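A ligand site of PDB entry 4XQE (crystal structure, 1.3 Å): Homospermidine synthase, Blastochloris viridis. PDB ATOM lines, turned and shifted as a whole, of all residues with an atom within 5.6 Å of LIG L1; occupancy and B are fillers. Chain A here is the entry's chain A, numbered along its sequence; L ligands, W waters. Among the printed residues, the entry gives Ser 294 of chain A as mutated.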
ATOM      1  N   ALA A 159     -13.581  21.569  18.207  1.00  0.00           N
ATOM      2  CA  ALA A 159     -14.023  22.808  17.578  1.00  0.00           C
ATOM      3  C   ALA A 159     -15.157  22.528  16.599  1.00  0.00           C
ATOM      4  O   ALA A 159     -16.164  23.227  16.605  1.00  0.00           O
ATOM      5  CB  ALA A 159     -12.873  23.440  16.860  1.00  0.00           C
ATOM      6  N   ASN A 160     -14.950  21.542  15.744  1.00  0.00           N
ATOM      7  CA  ASN A 160     -15.945  21.183  14.757  1.00  0.00           C
ATOM      8  C   ASN A 160     -15.653  19.754  14.353  1.00  0.00           C
ATOM      9  O   ASN A 160     -14.692  19.498  13.628  1.00  0.00           O
ATOM     10  CB  ASN A 160     -15.947  22.121  13.536  1.00  0.00           C
ATOM     11  CG  ASN A 160     -14.596  22.268  12.846  1.00  0.00           C
ATOM     12  OD1 ASN A 160     -13.582  22.621  13.460  1.00  0.00           O
ATOM     13  ND2 ASN A 160     -14.584  22.053  11.555  1.00  0.00           N
ATOM     14  N   PRO A 161     -16.437  18.786  14.836  1.00  0.00           N
ATOM     15  CA  PRO A 161     -17.640  18.930  15.659  1.00  0.00           C
ATOM     16  C   PRO A 161     -17.300  19.421  17.055  1.00  0.00           C
ATOM     17  O   PRO A 161     -16.182  19.212  17.561  1.00  0.00           O
ATOM     18  CB  PRO A 161     -18.144  17.485  15.754  1.00  0.00           C
ATOM     19  CG  PRO A 161     -16.892  16.641  15.579  1.00  0.00           C
ATOM     20  CD  PRO A 161     -16.117  17.384  14.546  1.00  0.00           C
ATOM     21  N   GLU A 208     -15.123  27.614   7.223  1.00  0.00           N
ATOM     22  CA  GLU A 208     -13.848  27.786   7.873  1.00  0.00           C
ATOM     23  C   GLU A 208     -12.791  28.218   6.862  1.00  0.00           C
ATOM     24  O   GLU A 208     -12.756  27.693   5.750  1.00  0.00           O
ATOM     25  CB  GLU A 208     -13.407  26.485   8.549  1.00  0.00           C
ATOM     26  CG  GLU A 208     -12.053  26.579   9.232  1.00  0.00           C
ATOM     27  CD  GLU A 208     -11.732  25.399  10.128  1.00  0.00           C
ATOM     28  OE1 GLU A 208     -12.422  24.378  10.059  1.00  0.00           O
ATOM     29  OE2 GLU A 208     -10.758  25.517  10.903  1.00  0.00           O
ATOM     30  N   TRP A 227      -3.318  20.687  12.141  1.00  0.00           N
ATOM     31  CA  TRP A 227      -3.763  19.687  13.103  1.00  0.00           C
ATOM     32  C   TRP A 227      -3.521  18.335  12.440  1.00  0.00           C
ATOM     33  O   TRP A 227      -2.996  18.303  11.330  1.00  0.00           O
ATOM     34  CB  TRP A 227      -5.254  19.865  13.473  1.00  0.00           C
ATOM     35  CG  TRP A 227      -6.181  19.795  12.285  1.00  0.00           C
ATOM     36  CD1 TRP A 227      -6.413  20.758  11.350  1.00  0.00           C
ATOM     37  CD2 TRP A 227      -7.004  18.668  11.914  1.00  0.00           C
ATOM     38  NE1 TRP A 227      -7.315  20.296  10.409  1.00  0.00           N
ATOM     39  CE2 TRP A 227      -7.692  19.024  10.754  1.00  0.00           C
ATOM     40  CE3 TRP A 227      -7.220  17.412  12.467  1.00  0.00           C
ATOM     41  CZ2 TRP A 227      -8.598  18.160  10.124  1.00  0.00           C
ATOM     42  CZ3 TRP A 227      -8.126  16.548  11.837  1.00  0.00           C
ATOM     43  CH2 TRP A 227      -8.786  16.922  10.672  1.00  0.00           C
ATOM     44  N   GLU A 235     -10.127  11.371   7.113  1.00  0.00           N
ATOM     45  CA  GLU A 235     -11.458  11.900   6.897  1.00  0.00           C
ATOM     46  C   GLU A 235     -11.612  12.431   5.474  1.00  0.00           C
ATOM     47  O   GLU A 235     -12.690  12.363   4.904  1.00  0.00           O
ATOM     48  CB  GLU A 235     -11.847  12.922   7.943  1.00  0.00           C
ATOM     49  CG  GLU A 235     -11.035  14.102   7.965  1.00  0.00           C
ATOM     50  CD  GLU A 235     -11.301  14.940   9.192  1.00  0.00           C
ATOM     51  OE1 GLU A 235     -11.564  14.365  10.281  1.00  0.00           O
ATOM     52  OE2 GLU A 235     -11.278  16.184   9.046  1.00  0.00           O
ATOM     53  N   VAL A 292     -15.522  17.916   3.352  1.00  0.00           N
ATOM     54  CA  VAL A 292     -15.012  16.860   4.208  1.00  0.00           C
ATOM     55  C   VAL A 292     -16.063  16.454   5.234  1.00  0.00           C
ATOM     56  O   VAL A 292     -16.743  17.301   5.795  1.00  0.00           O
ATOM     57  CB  VAL A 292     -13.723  17.318   4.883  1.00  0.00           C
ATOM     58  CG1 VAL A 292     -13.177  16.252   5.847  1.00  0.00           C
ATOM     59  CG2 VAL A 292     -12.685  17.653   3.828  1.00  0.00           C
ATOM     60  N   THR A 293     -16.214  15.150   5.427  1.00  0.00           N
ATOM     61  CA  THR A 293     -17.186  14.657   6.384  1.00  0.00           C
ATOM     62  C   THR A 293     -16.865  15.132   7.796  1.00  0.00           C
ATOM     63  O   THR A 293     -15.705  15.364   8.148  1.00  0.00           O
ATOM     64  CB  THR A 293     -17.260  13.148   6.370  1.00  0.00           C
ATOM     65  OG1 THR A 293     -18.336  12.752   7.247  1.00  0.00           O
ATOM     66  CG2 THR A 293     -15.963  12.513   6.846  1.00  0.00           C
ATOM     67  N   SER A 294     -17.905  15.258   8.592  1.00  0.00           N
ATOM     68  CA  SER A 294     -17.777  15.702   9.966  1.00  0.00           C
ATOM     69  C   SER A 294     -19.019  15.226  10.712  1.00  0.00           C
ATOM     70  O   SER A 294     -20.106  15.224  10.161  1.00  0.00           O
ATOM     71  CB  SER A 294     -17.666  17.222   9.997  1.00  0.00           C
ATOM     72  OG  SER A 294     -17.079  17.666  11.212  1.00  0.00           O
ATOM     73  N   GLU A 296     -20.801  16.642  12.940  1.00  0.00           N
ATOM     74  CA  GLU A 296     -21.858  17.615  13.182  1.00  0.00           C
ATOM     75  C   GLU A 296     -22.668  17.908  11.944  1.00  0.00           C
ATOM     76  O   GLU A 296     -23.772  18.445  12.041  1.00  0.00           O
ATOM     77  CB  GLU A 296     -21.331  18.892  13.814  1.00  0.00           C
ATOM     78  CG  GLU A 296     -20.663  19.854  12.874  1.00  0.00           C
ATOM     79  CD  GLU A 296     -19.253  19.486  12.495  1.00  0.00           C
ATOM     80  OE1 GLU A 296     -18.833  18.323  12.657  1.00  0.00           O
ATOM     81  OE2 GLU A 296     -18.522  20.399  12.024  1.00  0.00           O
ATOM     82  N   TYR A 321     -19.659  20.640   6.133  1.00  0.00           N
ATOM     83  CA  TYR A 321     -18.399  21.359   6.187  1.00  0.00           C
ATOM     84  C   TYR A 321     -18.107  22.000   4.849  1.00  0.00           C
ATOM     85  O   TYR A 321     -18.407  21.443   3.786  1.00  0.00           O
ATOM     86  CB  TYR A 321     -17.302  20.351   6.512  1.00  0.00           C
ATOM     87  CG  TYR A 321     -16.041  20.819   7.221  1.00  0.00           C
ATOM     88  CD1 TYR A 321     -15.856  22.133   7.651  1.00  0.00           C
ATOM     89  CD2 TYR A 321     -15.058  19.898   7.518  1.00  0.00           C
ATOM     90  CE1 TYR A 321     -14.670  22.517   8.316  1.00  0.00           C
ATOM     91  CE2 TYR A 321     -13.899  20.257   8.180  1.00  0.00           C
ATOM     92  CZ  TYR A 321     -13.708  21.555   8.583  1.00  0.00           C
ATOM     93  OH  TYR A 321     -12.538  21.866   9.265  1.00  0.00           O
ATOM     94  N   TYR A 323     -14.649  23.533   4.096  1.00  0.00           N
ATOM     95  CA  TYR A 323     -13.357  23.762   4.730  1.00  0.00           C
ATOM     96  C   TYR A 323     -12.322  24.278   3.778  1.00  0.00           C
ATOM     97  O   TYR A 323     -11.982  23.597   2.832  1.00  0.00           O
ATOM     98  CB  TYR A 323     -12.837  22.418   5.252  1.00  0.00           C
ATOM     99  CG  TYR A 323     -11.589  22.453   6.121  1.00  0.00           C
ATOM    100  CD1 TYR A 323     -11.195  23.610   6.789  1.00  0.00           C
ATOM    101  CD2 TYR A 323     -10.854  21.296   6.330  1.00  0.00           C
ATOM    102  CE1 TYR A 323     -10.079  23.580   7.639  1.00  0.00           C
ATOM    103  CE2 TYR A 323      -9.761  21.273   7.159  1.00  0.00           C
ATOM    104  CZ  TYR A 323      -9.373  22.403   7.812  1.00  0.00           C
ATOM    105  OH  TYR A 323      -8.285  22.343   8.635  1.00  0.00           O
ATOM    106  N   ASP A 359      -7.418  31.188  12.501  1.00  0.00           N
ATOM    107  CA  ASP A 359      -8.317  30.105  12.103  1.00  0.00           C
ATOM    108  C   ASP A 359      -9.726  30.666  12.234  1.00  0.00           C
ATOM    109  O   ASP A 359     -10.264  30.816  13.354  1.00  0.00           O
ATOM    110  CB  ASP A 359      -8.093  28.845  12.950  1.00  0.00           C
ATOM    111  CG  ASP A 359      -8.744  27.624  12.320  1.00  0.00           C
ATOM    112  OD1 ASP A 359      -9.810  27.775  11.688  1.00  0.00           O
ATOM    113  OD2 ASP A 359      -8.210  26.505  12.422  1.00  0.00           O
ATOM    114  N   LEU A 361     -13.353  30.272  11.990  1.00  0.00           N
ATOM    115  CA  LEU A 361     -14.201  29.088  12.070  1.00  0.00           C
ATOM    116  C   LEU A 361     -15.557  29.462  12.610  1.00  0.00           C
ATOM    117  O   LEU A 361     -15.660  29.955  13.740  1.00  0.00           O
ATOM    118  CB  LEU A 361     -13.539  28.044  12.969  1.00  0.00           C
ATOM    119  CG  LEU A 361     -14.364  26.809  13.337  1.00  0.00           C
ATOM    120  CD1 LEU A 361     -14.907  26.093  12.123  1.00  0.00           C
ATOM    121  CD2 LEU A 361     -13.509  25.883  14.160  1.00  0.00           C
ATOM    122  N   THR A 394      -5.605  26.766  15.531  1.00  0.00           N
ATOM    123  CA  THR A 394      -6.464  25.635  15.262  1.00  0.00           C
ATOM    124  C   THR A 394      -6.594  24.814  16.538  1.00  0.00           C
ATOM    125  O   THR A 394      -7.707  24.421  16.948  1.00  0.00           O
ATOM    126  CB  THR A 394      -5.879  24.788  14.127  1.00  0.00           C
ATOM    127  OG1 THR A 394      -5.700  25.623  12.979  1.00  0.00           O
ATOM    128  CG2 THR A 394      -6.800  23.646  13.772  1.00  0.00           C
ATOM    129  N   GLN A 397      -8.740  26.375  19.496  1.00  0.00           N
ATOM    130  CA  GLN A 397     -10.207  26.276  19.338  1.00  0.00           C
ATOM    131  C   GLN A 397     -10.694  24.890  19.754  1.00  0.00           C
ATOM    132  O   GLN A 397     -11.752  24.760  20.383  1.00  0.00           O
ATOM    133  CB  GLN A 397     -10.619  26.589  17.908  1.00  0.00           C
ATOM    134  CG  GLN A 397     -10.396  28.040  17.542  1.00  0.00           C
ATOM    135  CD  GLN A 397     -10.567  28.323  16.071  1.00  0.00           C
ATOM    136  OE1 GLN A 397     -10.304  27.476  15.218  1.00  0.00           O
ATOM    137  NE2 GLN A 397     -10.986  29.545  15.766  1.00  0.00           N
ATOM    138  N   VAL A 398      -9.906  23.862  19.470  1.00  0.00           N
ATOM    139  CA  VAL A 398     -10.265  22.508  19.811  1.00  0.00           C
ATOM    140  C   VAL A 398     -10.071  22.243  21.308  1.00  0.00           C
ATOM    141  O   VAL A 398     -10.992  21.747  21.973  1.00  0.00           O
ATOM    142  CB  VAL A 398      -9.462  21.478  19.009  1.00  0.00           C
ATOM    143  CG1 VAL A 398      -9.924  20.083  19.350  1.00  0.00           C
ATOM    144  CG2 VAL A 398      -9.605  21.734  17.507  1.00  0.00           C
HETATM  145  N1  LIG L   1     -11.039  23.340  12.745  1.00  0.00           N
HETATM  146  C1  LIG L   1     -10.270  22.276  12.145  1.00  0.00           C
HETATM  147  C2  LIG L   1     -10.655  20.912  12.721  1.00  0.00           C
HETATM  148  C3  LIG L   1     -11.253  19.995  11.664  1.00  0.00           C
HETATM  149  C4  LIG L   1     -11.696  18.633  12.210  1.00  0.00           C
HETATM  150  N2  LIG L   1     -12.046  17.785  11.111  1.00  0.00           N
HETATM  151  C5  LIG L   1     -13.363  17.640  10.604  1.00  0.00           C
HETATM  152  N3  LIG L   1     -13.677  16.806   9.505  1.00  0.00           N
HETATM  153  N4  LIG L   1     -14.366  18.244  11.112  1.00  0.00           N
HETATM  154  P1  LG2 L   2      -2.201  14.008  15.942  1.00  0.00           P
HETATM  155  O1  LG2 L   2      -2.055  13.217  14.656  1.00  0.00           O
HETATM  156  O2  LG2 L   2      -1.335  15.199  16.151  1.00  0.00           O
HETATM  157  O3  LG2 L   2      -1.969  13.049  17.195  1.00  0.00           O
HETATM  158  C1  LG2 L   2      -2.568  11.767  17.285  1.00  0.00           C
HETATM  159  C2  LG2 L   2      -1.904  11.129  18.374  1.00  0.00           C
HETATM  160  O4  LG2 L   2      -2.519   9.801  18.621  1.00  0.00           O
HETATM  161  C3  LG2 L   2      -0.411  10.673  18.208  1.00  0.00           C
HETATM  162  O5  LG2 L   2       0.532  11.447  18.995  1.00  0.00           O
HETATM  163  C4  LG2 L   2      -0.266   9.464  17.924  1.00  0.00           C
HETATM  164  O6  LG2 L   2       0.917   8.770  18.445  1.00  0.00           O
HETATM  165  C5  LG2 L   2      -1.583   8.923  18.665  1.00  0.00           C
HETATM  166  N1  LG2 L   2      -1.921   7.578  18.688  1.00  0.00           N
HETATM  167  C6  LG2 L   2      -1.874   6.841  17.561  1.00  0.00           C
HETATM  168  N2  LG2 L   2      -2.297   5.625  17.795  1.00  0.00           N
HETATM  169  C7  LG2 L   2      -2.645   5.559  19.128  1.00  0.00           C
HETATM  170  C8  LG2 L   2      -3.175   4.539  19.970  1.00  0.00           C
HETATM  171  N3  LG2 L   2      -3.431   3.251  19.444  1.00  0.00           N
HETATM  172  N4  LG2 L   2      -3.368   4.816  21.257  1.00  0.00           N
HETATM  173  C9  LG2 L   2      -3.115   6.005  21.753  1.00  0.00           C
HETATM  174  N5  LG2 L   2      -2.663   7.005  21.002  1.00  0.00           N
HETATM  175  C10 LG2 L   2      -2.405   6.810  19.689  1.00  0.00           C
HETATM  176  O7  LG2 L   2      -3.743  14.371  16.031  1.00  0.00           O
HETATM  177  P2  LG2 L   2      -4.444  15.624  16.753  1.00  0.00           P
HETATM  178  O8  LG2 L   2      -3.961  15.737  18.141  1.00  0.00           O
HETATM  179  O9  LG2 L   2      -4.297  16.875  15.911  1.00  0.00           O
HETATM  180  O10 LG2 L   2      -5.970  15.113  16.721  1.00  0.00           O
HETATM  181  C11 LG2 L   2      -6.338  14.157  17.710  1.00  0.00           C
HETATM  182  C12 LG2 L   2      -7.762  13.676  17.422  1.00  0.00           C
HETATM  183  O11 LG2 L   2      -8.576  14.682  17.504  1.00  0.00           O
HETATM  184  C13 LG2 L   2      -7.886  13.077  15.991  1.00  0.00           C
HETATM  185  O12 LG2 L   2      -8.651  11.953  15.969  1.00  0.00           O
HETATM  186  C14 LG2 L   2      -8.771  14.079  15.319  1.00  0.00           C
HETATM  187  O13 LG2 L   2      -9.275  13.723  14.031  1.00  0.00           O
HETATM  188  C15 LG2 L   2      -9.438  14.791  16.167  1.00  0.00           C
HETATM  189  N6  LG2 L   2      -9.646  16.184  15.988  1.00  0.00           N
HETATM  190  C16 LG2 L   2     -10.907  16.680  16.155  1.00  0.00           C
HETATM  191  C17 LG2 L   2     -11.127  18.038  15.983  1.00  0.00           C
HETATM  192  C18 LG2 L   2     -12.475  18.719  16.178  1.00  0.00           C
HETATM  193  O14 LG2 L   2     -12.558  19.935  16.117  1.00  0.00           O
HETATM  194  N7  LG2 L   2     -13.566  17.940  16.576  1.00  0.00           N
HETATM  195  C19 LG2 L   2     -10.076  18.875  15.668  1.00  0.00           C
HETATM  196  C20 LG2 L   2      -8.793  18.334  15.573  1.00  0.00           C
HETATM  197  C21 LG2 L   2      -8.623  16.971  15.737  1.00  0.00           C
HETATM  198  O   HOH W   1      -9.968  24.628  15.048  1.00  0.00           O
HETATM  199  O   HOH W   2     -11.533  14.939  13.073  1.00  0.00           O
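The side-chain carboxylate of Glu 235 lies within salt-bridge range of a nitrogen (N3) of LIG L1 (2.5 Å). N4 of LIG L1 lies within hydrogen-bond range of O of Asn 160 (2.8 Å). N1 of LIG L1 is in hydrogen-bond range of OD1 of Asn 160. A nitrogen (N4) of LIG L1 is in hydrogen-bond range of the side-chain hydroxyl of Ser 294. The backbone carbonyl oxygen (O) of Thr 293 sits at hydrogen-bond distance from a nitrogen (N3) of LIG L1, at 2.8 Å. The side-chain carboxylate of Glu 208 lies within salt-bridge range of a nitrogen (N1) of LIG L1. O14 of LG2 L2 sits at hydrogen-bond distance from N of Asn 160 (2.9 Å). The backbone carbonyl oxygen (O) of Pro 161 sits at hydrogen-bond distance from a nitrogen (N7) of LG2 L2 (3.1 Å). N of Ala 159 is in hydrogen-bond range of O14 of LG2 L2 (2.8 Å).
The side-chain amide nitrogen (ND2) of Asn 160 is in hydrogen-bond range of the side-chain hydroxyl (OH) of Tyr 321 (3.1 Å). The side-chain carboxylate (OE2) of Glu 296 sits close to the side-chain hydroxyl (OG) of Ser 294 (3.2 Å). The side-chain carboxylate (OE1) of Glu 208 sits at hydrogen-bond distance from the side-chain hydroxyl (OH) of Tyr 321 (2.6 Å). The side-chain carboxylate of Glu 208 lies close to the side-chain carboxylate of Asp 359. NE1 of Trp 227 lies within hydrogen-bond range of OH of Tyr 323.
CD of Pro 161 touches N4 of LIG L1, 3.9 Å away. Trp 227 touches LIG L1. Val 292 touches LIG L1. Tyr 321 touches LIG L1. CD2 of Leu 361 touches N1 of LIG L1, 3.8 Å away. Ten residues have an atom within 4 Å of LIG L1: Asn 160, Pro 161, Glu 208, Trp 227, Glu 235, Val 292, Thr 293, Ser 294, Tyr 321 and Leu 361.
Water W1 lies within hydrogen-bond range of a nitrogen (N1) of LIG L1 (2.8 Å), the side-chain amide oxygen of Gln 397 (2.9 Å) and the backbone carbonyl oxygen of Thr 394 (3.0 Å). Water W2 lies within hydrogen-bond range of an oxygen (O13) of LG2 L2 (2.7 Å), the side-chain carboxylate (OE1) of Glu 235 (2.9 Å) and a nitrogen (N2) of LIG L1 (3.5 Å).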
